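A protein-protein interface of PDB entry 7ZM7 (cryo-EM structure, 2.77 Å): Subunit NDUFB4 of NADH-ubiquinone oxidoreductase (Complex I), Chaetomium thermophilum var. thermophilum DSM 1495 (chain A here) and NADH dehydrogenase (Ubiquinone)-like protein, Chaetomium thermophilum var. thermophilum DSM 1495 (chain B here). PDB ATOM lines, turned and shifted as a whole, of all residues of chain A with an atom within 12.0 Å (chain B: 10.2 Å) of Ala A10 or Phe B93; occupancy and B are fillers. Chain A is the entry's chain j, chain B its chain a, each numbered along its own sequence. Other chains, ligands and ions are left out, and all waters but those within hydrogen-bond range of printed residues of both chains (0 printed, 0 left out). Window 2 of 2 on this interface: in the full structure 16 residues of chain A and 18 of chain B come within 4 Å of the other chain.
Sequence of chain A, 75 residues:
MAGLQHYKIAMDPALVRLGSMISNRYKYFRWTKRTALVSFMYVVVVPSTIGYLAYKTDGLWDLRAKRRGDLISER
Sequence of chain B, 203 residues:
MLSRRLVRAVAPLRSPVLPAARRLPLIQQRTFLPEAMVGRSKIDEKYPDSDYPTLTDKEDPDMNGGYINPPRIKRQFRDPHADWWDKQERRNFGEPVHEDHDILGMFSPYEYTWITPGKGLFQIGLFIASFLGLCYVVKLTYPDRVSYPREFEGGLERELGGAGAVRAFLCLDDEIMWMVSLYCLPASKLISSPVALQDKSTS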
ATOM      1  N   HIS A   6       9.463  41.941 -27.261  1.00  0.00           N
ATOM      2  CA  HIS A   6      10.401  41.406 -26.260  1.00  0.00           C
ATOM      3  C   HIS A   6      11.375  40.431 -26.933  1.00  0.00           C
ATOM      4  O   HIS A   6      11.222  40.189 -28.134  1.00  0.00           O
ATOM      5  CB  HIS A   6       9.566  40.782 -25.146  1.00  0.00           C
ATOM      6  CG  HIS A   6       8.559  39.783 -25.600  1.00  0.00           C
ATOM      7  ND1 HIS A   6       8.873  38.458 -25.800  1.00  0.00           N
ATOM      8  CD2 HIS A   6       7.242  39.902 -25.855  1.00  0.00           C
ATOM      9  CE1 HIS A   6       7.799  37.806 -26.182  1.00  0.00           C
ATOM     10  NE2 HIS A   6       6.784  38.668 -26.222  1.00  0.00           N
ATOM     11  N   TYR A   7      12.368  39.961 -26.189  1.00  0.00           N
ATOM     12  CA  TYR A   7      13.343  38.988 -26.708  1.00  0.00           C
ATOM     13  C   TYR A   7      12.648  37.633 -26.801  1.00  0.00           C
ATOM     14  O   TYR A   7      11.619  37.439 -26.154  1.00  0.00           O
ATOM     15  CB  TYR A   7      14.558  38.929 -25.791  1.00  0.00           C
ATOM     16  CG  TYR A   7      15.445  40.145 -25.753  1.00  0.00           C
ATOM     17  CD1 TYR A   7      16.390  40.363 -26.735  1.00  0.00           C
ATOM     18  CD2 TYR A   7      15.384  41.046 -24.705  1.00  0.00           C
ATOM     19  CE1 TYR A   7      17.224  41.466 -26.701  1.00  0.00           C
ATOM     20  CE2 TYR A   7      16.212  42.155 -24.654  1.00  0.00           C
ATOM     21  CZ  TYR A   7      17.136  42.366 -25.657  1.00  0.00           C
ATOM     22  OH  TYR A   7      17.961  43.452 -25.631  1.00  0.00           O
ATOM     23  N   LYS A   8      13.246  36.687 -27.520  1.00  0.00           N
ATOM     24  CA  LYS A   8      12.628  35.349 -27.703  1.00  0.00           C
ATOM     25  C   LYS A   8      12.661  34.537 -26.403  1.00  0.00           C
ATOM     26  O   LYS A   8      13.728  34.452 -25.792  1.00  0.00           O
ATOM     27  CB  LYS A   8      13.304  34.627 -28.870  1.00  0.00           C
ATOM     28  CG  LYS A   8      13.387  35.440 -30.155  1.00  0.00           C
ATOM     29  CD  LYS A   8      14.108  34.724 -31.273  1.00  0.00           C
ATOM     30  CE  LYS A   8      14.352  35.612 -32.475  1.00  0.00           C
ATOM     31  NZ  LYS A   8      13.096  36.226 -32.965  1.00  0.00           N
ATOM     32  N   ILE A   9      11.517  33.979 -26.000  1.00  0.00           N
ATOM     33  CA  ILE A   9      11.410  33.163 -24.751  1.00  0.00           C
ATOM     34  C   ILE A   9      10.886  31.785 -25.132  1.00  0.00           C
ATOM     35  O   ILE A   9       9.925  31.733 -25.908  1.00  0.00           O
ATOM     36  CB  ILE A   9      10.455  33.827 -23.740  1.00  0.00           C
ATOM     37  CG1 ILE A   9      10.924  35.229 -23.362  1.00  0.00           C
ATOM     38  CG2 ILE A   9      10.303  32.956 -22.503  1.00  0.00           C
ATOM     39  CD1 ILE A   9      12.104  35.217 -22.429  1.00  0.00           C
ATOM     40  N   ALA A  10      11.531  30.721 -24.667  1.00  0.00           N
ATOM     41  CA  ALA A  10      11.004  29.362 -24.895  1.00  0.00           C
ATOM     42  C   ALA A  10       9.786  29.213 -24.001  1.00  0.00           C
ATOM     43  O   ALA A  10       9.910  28.557 -22.958  1.00  0.00           O
ATOM     44  CB  ALA A  10      12.033  28.349 -24.487  1.00  0.00           C
ATOM     45  N   MET A  11       8.673  29.835 -24.383  1.00  0.00           N
ATOM     46  CA  MET A  11       7.498  29.801 -23.502  1.00  0.00           C
ATOM     47  C   MET A  11       7.131  28.335 -23.357  1.00  0.00           C
ATOM     48  O   MET A  11       7.000  27.649 -24.386  1.00  0.00           O
ATOM     49  CB  MET A  11       6.363  30.596 -24.133  1.00  0.00           C
ATOM     50  CG  MET A  11       5.670  31.523 -23.151  1.00  0.00           C
ATOM     51  SD  MET A  11       6.824  32.532 -22.184  1.00  0.00           S
ATOM     52  CE  MET A  11       5.686  33.426 -21.128  1.00  0.00           C
ATOM     53  N   ASP A  12       6.981  27.886 -22.119  1.00  0.00           N
ATOM     54  CA  ASP A  12       6.713  26.460 -21.858  1.00  0.00           C
ATOM     55  C   ASP A  12       5.204  26.211 -21.943  1.00  0.00           C
ATOM     56  O   ASP A  12       4.481  26.809 -21.134  1.00  0.00           O
ATOM     57  CB  ASP A  12       7.210  26.115 -20.471  1.00  0.00           C
ATOM     58  CG  ASP A  12       7.669  24.692 -20.343  1.00  0.00           C
ATOM     59  OD1 ASP A  12       6.842  23.797 -20.582  1.00  0.00           O
ATOM     60  OD2 ASP A  12       8.850  24.513 -20.010  1.00  0.00           O
ATOM     61  N   PRO A  13       4.676  25.342 -22.836  1.00  0.00           N
ATOM     62  CA  PRO A  13       3.237  25.068 -22.824  1.00  0.00           C
ATOM     63  C   PRO A  13       2.742  24.637 -21.462  1.00  0.00           C
ATOM     64  O   PRO A  13       1.605  24.943 -21.094  1.00  0.00           O
ATOM     65  CB  PRO A  13       3.085  23.951 -23.866  1.00  0.00           C
ATOM     66  CG  PRO A  13       4.322  24.011 -24.680  1.00  0.00           C
ATOM     67  CD  PRO A  13       5.395  24.453 -23.758  1.00  0.00           C
ATOM     68  N   ALA A  14       3.584  23.948 -20.698  1.00  0.00           N
ATOM     69  CA  ALA A  14       3.186  23.460 -19.388  1.00  0.00           C
ATOM     70  C   ALA A  14       3.045  24.600 -18.400  1.00  0.00           C
ATOM     71  O   ALA A  14       2.068  24.670 -17.650  1.00  0.00           O
ATOM     72  CB  ALA A  14       4.199  22.436 -18.890  1.00  0.00           C
ATOM     73  N   LEU A  15       4.021  25.497 -18.372  1.00  0.00           N
ATOM     74  CA  LEU A  15       4.029  26.552 -17.369  1.00  0.00           C
ATOM     75  C   LEU A  15       3.013  27.638 -17.691  1.00  0.00           C
ATOM     76  O   LEU A  15       2.440  28.245 -16.782  1.00  0.00           O
ATOM     77  CB  LEU A  15       5.432  27.120 -17.255  1.00  0.00           C
ATOM     78  CG  LEU A  15       6.421  26.094 -16.729  1.00  0.00           C
ATOM     79  CD1 LEU A  15       7.820  26.615 -16.862  1.00  0.00           C
ATOM     80  CD2 LEU A  15       6.124  25.772 -15.279  1.00  0.00           C
ATOM     81  N   VAL A  16       2.770  27.892 -18.975  1.00  0.00           N
ATOM     82  CA  VAL A  16       1.757  28.868 -19.361  1.00  0.00           C
ATOM     83  C   VAL A  16       0.384  28.443 -18.856  1.00  0.00           C
ATOM     84  O   VAL A  16      -0.364  29.244 -18.288  1.00  0.00           O
ATOM     85  CB  VAL A  16       1.771  29.068 -20.885  1.00  0.00           C
ATOM     86  CG1 VAL A  16       0.576  29.834 -21.346  1.00  0.00           C
ATOM     87  CG2 VAL A  16       3.009  29.806 -21.282  1.00  0.00           C
ATOM     88  N   ARG A  17       0.039  27.176 -19.038  1.00  0.00           N
ATOM     89  CA  ARG A  17      -1.260  26.715 -18.580  1.00  0.00           C
ATOM     90  C   ARG A  17      -1.327  26.625 -17.059  1.00  0.00           C
ATOM     91  O   ARG A  17      -2.417  26.704 -16.486  1.00  0.00           O
ATOM     92  CB  ARG A  17      -1.582  25.373 -19.231  1.00  0.00           C
ATOM     93  CG  ARG A  17      -0.739  24.231 -18.763  1.00  0.00           C
ATOM     94  CD  ARG A  17      -1.333  22.914 -19.198  1.00  0.00           C
ATOM     95  NE  ARG A  17      -0.784  22.462 -20.471  1.00  0.00           N
ATOM     96  CZ  ARG A  17       0.222  21.601 -20.583  1.00  0.00           C
ATOM     97  NH1 ARG A  17       0.664  21.250 -21.781  1.00  0.00           N
ATOM     98  NH2 ARG A  17       0.780  21.085 -19.494  1.00  0.00           N
ATOM     99  N   LEU A  18      -0.188  26.451 -16.391  1.00  0.00           N
ATOM    100  CA  LEU A  18      -0.164  26.538 -14.938  1.00  0.00           C
ATOM    101  C   LEU A  18      -0.490  27.943 -14.457  1.00  0.00           C
ATOM    102  O   LEU A  18      -1.215  28.115 -13.471  1.00  0.00           O
ATOM    103  CB  LEU A  18       1.199  26.116 -14.408  1.00  0.00           C
ATOM    104  CG  LEU A  18       1.417  26.332 -12.913  1.00  0.00           C
ATOM    105  CD1 LEU A  18       0.469  25.494 -12.100  1.00  0.00           C
ATOM    106  CD2 LEU A  18       2.839  26.057 -12.546  1.00  0.00           C
ATOM    107  N   ARG B  78      14.423  13.181  -8.054  1.00  0.00           N
ATOM    108  CA  ARG B  78      14.674  12.741  -9.408  1.00  0.00           C
ATOM    109  C   ARG B  78      16.129  12.339  -9.555  1.00  0.00           C
ATOM    110  O   ARG B  78      16.939  12.481  -8.635  1.00  0.00           O
ATOM    111  CB  ARG B  78      14.324  13.835 -10.406  1.00  0.00           C
ATOM    112  CG  ARG B  78      12.943  14.370 -10.241  1.00  0.00           C
ATOM    113  CD  ARG B  78      12.512  15.090 -11.459  1.00  0.00           C
ATOM    114  NE  ARG B  78      11.093  15.348 -11.394  1.00  0.00           N
ATOM    115  CZ  ARG B  78      10.371  15.803 -12.400  1.00  0.00           C
ATOM    116  NH1 ARG B  78       9.072  15.992 -12.239  1.00  0.00           N
ATOM    117  NH2 ARG B  78      10.949  16.069 -13.562  1.00  0.00           N
ATOM    118  N   ASP B  83      18.717  12.841 -18.742  1.00  0.00           N
ATOM    119  CA  ASP B  83      18.924  13.740 -19.874  1.00  0.00           C
ATOM    120  C   ASP B  83      18.001  14.949 -19.765  1.00  0.00           C
ATOM    121  O   ASP B  83      17.289  15.314 -20.696  1.00  0.00           O
ATOM    122  CB  ASP B  83      18.707  12.998 -21.185  1.00  0.00           C
ATOM    123  CG  ASP B  83      19.898  12.167 -21.583  1.00  0.00           C
ATOM    124  OD1 ASP B  83      21.032  12.566 -21.248  1.00  0.00           O
ATOM    125  OD2 ASP B  83      19.699  11.117 -22.228  1.00  0.00           O
ATOM    126  N   TRP B  84      18.032  15.569 -18.594  1.00  0.00           N
ATOM    127  CA  TRP B  84      17.136  16.675 -18.317  1.00  0.00           C
ATOM    128  C   TRP B  84      17.400  17.842 -19.258  1.00  0.00           C
ATOM    129  O   TRP B  84      18.545  18.256 -19.458  1.00  0.00           O
ATOM    130  CB  TRP B  84      17.300  17.139 -16.876  1.00  0.00           C
ATOM    131  CG  TRP B  84      17.078  16.105 -15.858  1.00  0.00           C
ATOM    132  CD1 TRP B  84      17.962  15.694 -14.920  1.00  0.00           C
ATOM    133  CD2 TRP B  84      15.885  15.361 -15.641  1.00  0.00           C
ATOM    134  NE1 TRP B  84      17.404  14.736 -14.134  1.00  0.00           N
ATOM    135  CE2 TRP B  84      16.123  14.512 -14.555  1.00  0.00           C
ATOM    136  CE3 TRP B  84      14.634  15.331 -16.260  1.00  0.00           C
ATOM    137  CZ2 TRP B  84      15.163  13.639 -14.073  1.00  0.00           C
ATOM    138  CZ3 TRP B  84      13.688  14.469 -15.783  1.00  0.00           C
ATOM    139  CH2 TRP B  84      13.956  13.634 -14.699  1.00  0.00           C
ATOM    140  N   TRP B  85      16.327  18.387 -19.823  1.00  0.00           N
ATOM    141  CA  TRP B  85      16.464  19.592 -20.627  1.00  0.00           C
ATOM    142  C   TRP B  85      17.015  20.730 -19.789  1.00  0.00           C
ATOM    143  O   TRP B  85      17.749  21.587 -20.290  1.00  0.00           O
ATOM    144  CB  TRP B  85      15.119  19.973 -21.223  1.00  0.00           C
ATOM    145  CG  TRP B  85      15.090  21.332 -21.761  1.00  0.00           C
ATOM    146  CD1 TRP B  85      15.468  21.724 -23.000  1.00  0.00           C
ATOM    147  CD2 TRP B  85      14.679  22.506 -21.070  1.00  0.00           C
ATOM    148  NE1 TRP B  85      15.307  23.071 -23.137  1.00  0.00           N
ATOM    149  CE2 TRP B  85      14.821  23.579 -21.962  1.00  0.00           C
ATOM    150  CE3 TRP B  85      14.198  22.752 -19.785  1.00  0.00           C
ATOM    151  CZ2 TRP B  85      14.507  24.878 -21.612  1.00  0.00           C
ATOM    152  CZ3 TRP B  85      13.886  24.036 -19.438  1.00  0.00           C
ATOM    153  CH2 TRP B  85      14.041  25.090 -20.349  1.00  0.00           C
ATOM    154  N   ASP B  86      16.663  20.751 -18.514  1.00  0.00           N
ATOM    155  CA  ASP B  86      17.235  21.654 -17.528  1.00  0.00           C
ATOM    156  C   ASP B  86      17.895  20.793 -16.464  1.00  0.00           C
ATOM    157  O   ASP B  86      17.232  20.276 -15.567  1.00  0.00           O
ATOM    158  CB  ASP B  86      16.183  22.573 -16.934  1.00  0.00           C
ATOM    159  CG  ASP B  86      16.784  23.594 -16.021  1.00  0.00           C
ATOM    160  OD1 ASP B  86      17.415  24.544 -16.510  1.00  0.00           O
ATOM    161  OD2 ASP B  86      16.621  23.458 -14.803  1.00  0.00           O
ATOM    162  N   LYS B  87      19.239  20.649 -16.618  1.00  0.00           N
ATOM    163  CA  LYS B  87      19.980  19.746 -15.701  1.00  0.00           C
ATOM    164  C   LYS B  87      19.964  20.293 -14.279  1.00  0.00           C
ATOM    165  O   LYS B  87      19.889  19.461 -13.359  1.00  0.00           O
ATOM    166  CB  LYS B  87      21.414  19.536 -16.200  1.00  0.00           C
ATOM    167  CG  LYS B  87      21.533  18.846 -17.552  1.00  0.00           C
ATOM    168  CD  LYS B  87      22.963  18.692 -18.018  1.00  0.00           C
ATOM    169  CE  LYS B  87      23.809  17.870 -17.068  1.00  0.00           C
ATOM    170  NZ  LYS B  87      23.308  16.481 -16.951  1.00  0.00           N
ATOM    171  N   GLU B  89      17.708  22.046 -12.456  1.00  0.00           N
ATOM    172  CA  GLU B  89      16.461  21.813 -11.746  1.00  0.00           C
ATOM    173  C   GLU B  89      15.885  20.433 -11.995  1.00  0.00           C
ATOM    174  O   GLU B  89      14.891  20.077 -11.358  1.00  0.00           O
ATOM    175  CB  GLU B  89      15.427  22.865 -12.144  1.00  0.00           C
ATOM    176  CG  GLU B  89      15.730  24.290 -11.721  1.00  0.00           C
ATOM    177  CD  GLU B  89      15.683  24.493 -10.211  1.00  0.00           C
ATOM    178  OE1 GLU B  89      14.883  23.802  -9.545  1.00  0.00           O
ATOM    179  OE2 GLU B  89      16.426  25.353  -9.689  1.00  0.00           O
ATOM    180  N   ARG B  90      16.479  19.657 -12.901  1.00  0.00           N
ATOM    181  CA  ARG B  90      16.035  18.306 -13.245  1.00  0.00           C
ATOM    182  C   ARG B  90      14.615  18.314 -13.811  1.00  0.00           C
ATOM    183  O   ARG B  90      13.694  17.708 -13.271  1.00  0.00           O
ATOM    184  CB  ARG B  90      16.148  17.373 -12.045  1.00  0.00           C
ATOM    185  CG  ARG B  90      17.519  17.359 -11.447  1.00  0.00           C
ATOM    186  CD  ARG B  90      17.512  16.692 -10.124  1.00  0.00           C
ATOM    187  NE  ARG B  90      18.803  16.783  -9.471  1.00  0.00           N
ATOM    188  CZ  ARG B  90      19.044  16.305  -8.261  1.00  0.00           C
ATOM    189  NH1 ARG B  90      18.075  15.714  -7.587  1.00  0.00           N
ATOM    190  NH2 ARG B  90      20.246  16.418  -7.730  1.00  0.00           N
ATOM    191  N   ARG B  91      14.470  18.994 -14.942  1.00  0.00           N
ATOM    192  CA  ARG B  91      13.183  19.186 -15.585  1.00  0.00           C
ATOM    193  C   ARG B  91      13.349  18.985 -17.085  1.00  0.00           C
ATOM    194  O   ARG B  91      14.403  19.292 -17.639  1.00  0.00           O
ATOM    195  CB  ARG B  91      12.628  20.595 -15.273  1.00  0.00           C
ATOM    196  CG  ARG B  91      11.221  20.859 -15.765  1.00  0.00           C
ATOM    197  CD  ARG B  91      10.744  22.258 -15.434  1.00  0.00           C
ATOM    198  NE  ARG B  91       9.365  22.449 -15.861  1.00  0.00           N
ATOM    199  CZ  ARG B  91       9.003  22.892 -17.055  1.00  0.00           C
ATOM    200  NH1 ARG B  91       9.924  23.213 -17.946  1.00  0.00           N
ATOM    201  NH2 ARG B  91       7.720  23.021 -17.357  1.00  0.00           N
ATOM    202  N   ASN B  92      12.328  18.451 -17.738  1.00  0.00           N
ATOM    203  CA  ASN B  92      12.293  18.442 -19.195  1.00  0.00           C
ATOM    204  C   ASN B  92      11.340  19.520 -19.673  1.00  0.00           C
ATOM    205  O   ASN B  92      10.477  19.980 -18.926  1.00  0.00           O
ATOM    206  CB  ASN B  92      11.862  17.087 -19.749  1.00  0.00           C
ATOM    207  CG  ASN B  92      12.940  16.049 -19.643  1.00  0.00           C
ATOM    208  OD1 ASN B  92      14.121  16.341 -19.800  1.00  0.00           O
ATOM    209  ND2 ASN B  92      12.538  14.820 -19.378  1.00  0.00           N
ATOM    210  N   PHE B  93      11.495  19.916 -20.930  1.00  0.00           N
ATOM    211  CA  PHE B  93      10.850  21.136 -21.387  1.00  0.00           C
ATOM    212  C   PHE B  93       9.329  21.134 -21.248  1.00  0.00           C
ATOM    213  O   PHE B  93       8.770  22.003 -20.579  1.00  0.00           O
ATOM    214  CB  PHE B  93      11.215  21.445 -22.826  1.00  0.00           C
ATOM    215  CG  PHE B  93      10.695  22.761 -23.281  1.00  0.00           C
ATOM    216  CD1 PHE B  93      11.146  23.924 -22.705  1.00  0.00           C
ATOM    217  CD2 PHE B  93       9.717  22.835 -24.250  1.00  0.00           C
ATOM    218  CE1 PHE B  93      10.648  25.132 -23.108  1.00  0.00           C
ATOM    219  CE2 PHE B  93       9.227  24.041 -24.658  1.00  0.00           C
ATOM    220  CZ  PHE B  93       9.691  25.185 -24.087  1.00  0.00           C
ATOM    221  N   GLY B  94       8.635  20.193 -21.845  1.00  0.00           N
ATOM    222  CA  GLY B  94       7.203  20.363 -21.759  1.00  0.00           C
ATOM    223  C   GLY B  94       6.482  19.553 -20.711  1.00  0.00           C
ATOM    224  O   GLY B  94       5.261  19.411 -20.805  1.00  0.00           O
ATOM    225  N   GLU B  95       7.244  19.072 -19.725  1.00  0.00           N
ATOM    226  CA  GLU B  95       6.701  18.141 -18.703  1.00  0.00           C
ATOM    227  C   GLU B  95       5.573  18.775 -17.892  1.00  0.00           C
ATOM    228  O   GLU B  95       5.687  19.977 -17.589  1.00  0.00           O
ATOM    229  CB  GLU B  95       7.828  17.612 -17.811  1.00  0.00           C
ATOM    230  CG  GLU B  95       8.240  18.546 -16.691  1.00  0.00           C
ATOM    231  CD  GLU B  95       9.227  17.920 -15.724  1.00  0.00           C
ATOM    232  OE1 GLU B  95       9.287  18.374 -14.566  1.00  0.00           O
ATOM    233  OE2 GLU B  95       9.936  16.982 -16.136  1.00  0.00           O
ATOM    234  N   PRO B  96       4.484  18.053 -17.517  1.00  0.00           N
ATOM    235  CA  PRO B  96       3.488  18.655 -16.634  1.00  0.00           C
ATOM    236  C   PRO B  96       4.075  18.982 -15.277  1.00  0.00           C
ATOM    237  O   PRO B  96       5.016  18.341 -14.809  1.00  0.00           O
ATOM    238  CB  PRO B  96       2.418  17.567 -16.523  1.00  0.00           C
ATOM    239  CG  PRO B  96       3.144  16.316 -16.793  1.00  0.00           C
ATOM    240  CD  PRO B  96       4.150  16.659 -17.838  1.00  0.00           C
ATOM    241  N   VAL B  97       3.493  19.983 -14.634  1.00  0.00           N
ATOM    242  CA  VAL B  97       3.982  20.481 -13.358  1.00  0.00           C
ATOM    243  C   VAL B  97       2.855  20.456 -12.340  1.00  0.00           C
ATOM    244  O   VAL B  97       1.711  20.792 -12.658  1.00  0.00           O
ATOM    245  CB  VAL B  97       4.585  21.896 -13.505  1.00  0.00           C
ATOM    246  CG1 VAL B  97       5.846  21.834 -14.330  1.00  0.00           C
ATOM    247  CG2 VAL B  97       3.608  22.804 -14.208  1.00  0.00           C
ATOM    248  N   HIS B 101       4.414  23.828  -7.863  1.00  0.00           N
ATOM    249  CA  HIS B 101       5.750  23.902  -8.513  1.00  0.00           C
ATOM    250  C   HIS B 101       6.710  24.827  -7.756  1.00  0.00           C
ATOM    251  O   HIS B 101       7.907  24.494  -7.720  1.00  0.00           O
ATOM    252  CB  HIS B 101       5.569  24.291  -9.987  1.00  0.00           C
ATOM    253  CG  HIS B 101       6.796  24.181 -10.827  1.00  0.00           C
ATOM    254  ND1 HIS B 101       7.188  22.994 -11.402  1.00  0.00           N
ATOM    255  CD2 HIS B 101       7.702  25.105 -11.212  1.00  0.00           C
ATOM    256  CE1 HIS B 101       8.286  23.189 -12.104  1.00  0.00           C
ATOM    257  NE2 HIS B 101       8.622  24.476 -12.000  1.00  0.00           N
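O of Ala A10 touches CE1 of Phe B93 (3.5 Å).
O of Met A11 touches CZ of Phe B93, at 3.7 Å.
Asp A12 touches Gly B94.
Phe B93 touches Pro A13.
Ala A14 touches Arg B91.
Gly B94 touches Ala A14.
O of Glu B95 touches CB of Ala A14, 3.2 Å away.
Arg B91 touches Leu A15.
CD2 of Leu A18 touches CG2 of Val B97, at 3.7 Å.
Ala A10 touches one residue of chain B.
Phe B93 touches four residues of chain A.
No residue of chain B comes within 4 Å of Ile A9.
Of chain B, only Arg B91, Phe B93 and Gly B94 come within 4 Å of Asp A12.
No residue of chain A comes within 4 Å of Trp B85.
No residue of chain A comes within 4 Å of Asn B92.
Of chain A, only Asp A12 (3.6 Å) and Ala A14 (3.7 Å) come within 4 Å of Gly B94.
Of the printed residues of chain A, Val B97 touches Leu A18.
Of the printed residues of chain B, Pro A13 touches Phe B93 (3.96 Å).
Lys B87 touches none of the printed residues of chain A.
The nearest residue of chain B that does not touch Ala A10 is Trp B85 (5.1 Å).
The nearest printed residue of chain B that does not touch Ala A14 is Val B97 (4.2 Å).
The side-chain carboxylate of Asp A12 lies within salt-bridge range of the guanidinium group of Arg B91, at 2.7 Å.
O of Phe B93 lies close to OD2 of Asp A12 (2.6 Å).
The side-chain carboxylate of Glu B95 is in salt-bridge range of the guanidinium group of Arg B78, at 2.9 Å.
N of Asp B86 lies within hydrogen-bond range of O of Arg B91, at 2.8 Å.
The backbone carbonyl oxygen (O) of Phe B93 sits at hydrogen-bond distance from the guanidinium group (NH1) of Arg B91 (3.1 Å).
N of Asn B92 is in hydrogen-bond range of OE2 of Glu B95, 3.2 Å away.
The backbone NH of Ala A14 sits close to the side-chain carboxylate of Asp A12 (3.3 Å).
The backbone carbonyl oxygen (O) of Pro A13 lies close to the guanidinium group (NE) of Arg A17, at 3.5 Å.
Hydrophobic or aromatic side chains of chain A that line the printed part of chain B: Ala A10, Pro A13, Ala A14, Leu A15 and Leu A18.
Hydrophobic or aromatic side chains of chain B within 4 Å of the printed part of chain A: Phe B93 and Val B97.
Among the printed residues, Asp or Glu carboxylates within 4 Å of a Lys or Arg side-chain nitrogen of the other chain: Asp A12 with Arg B91.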
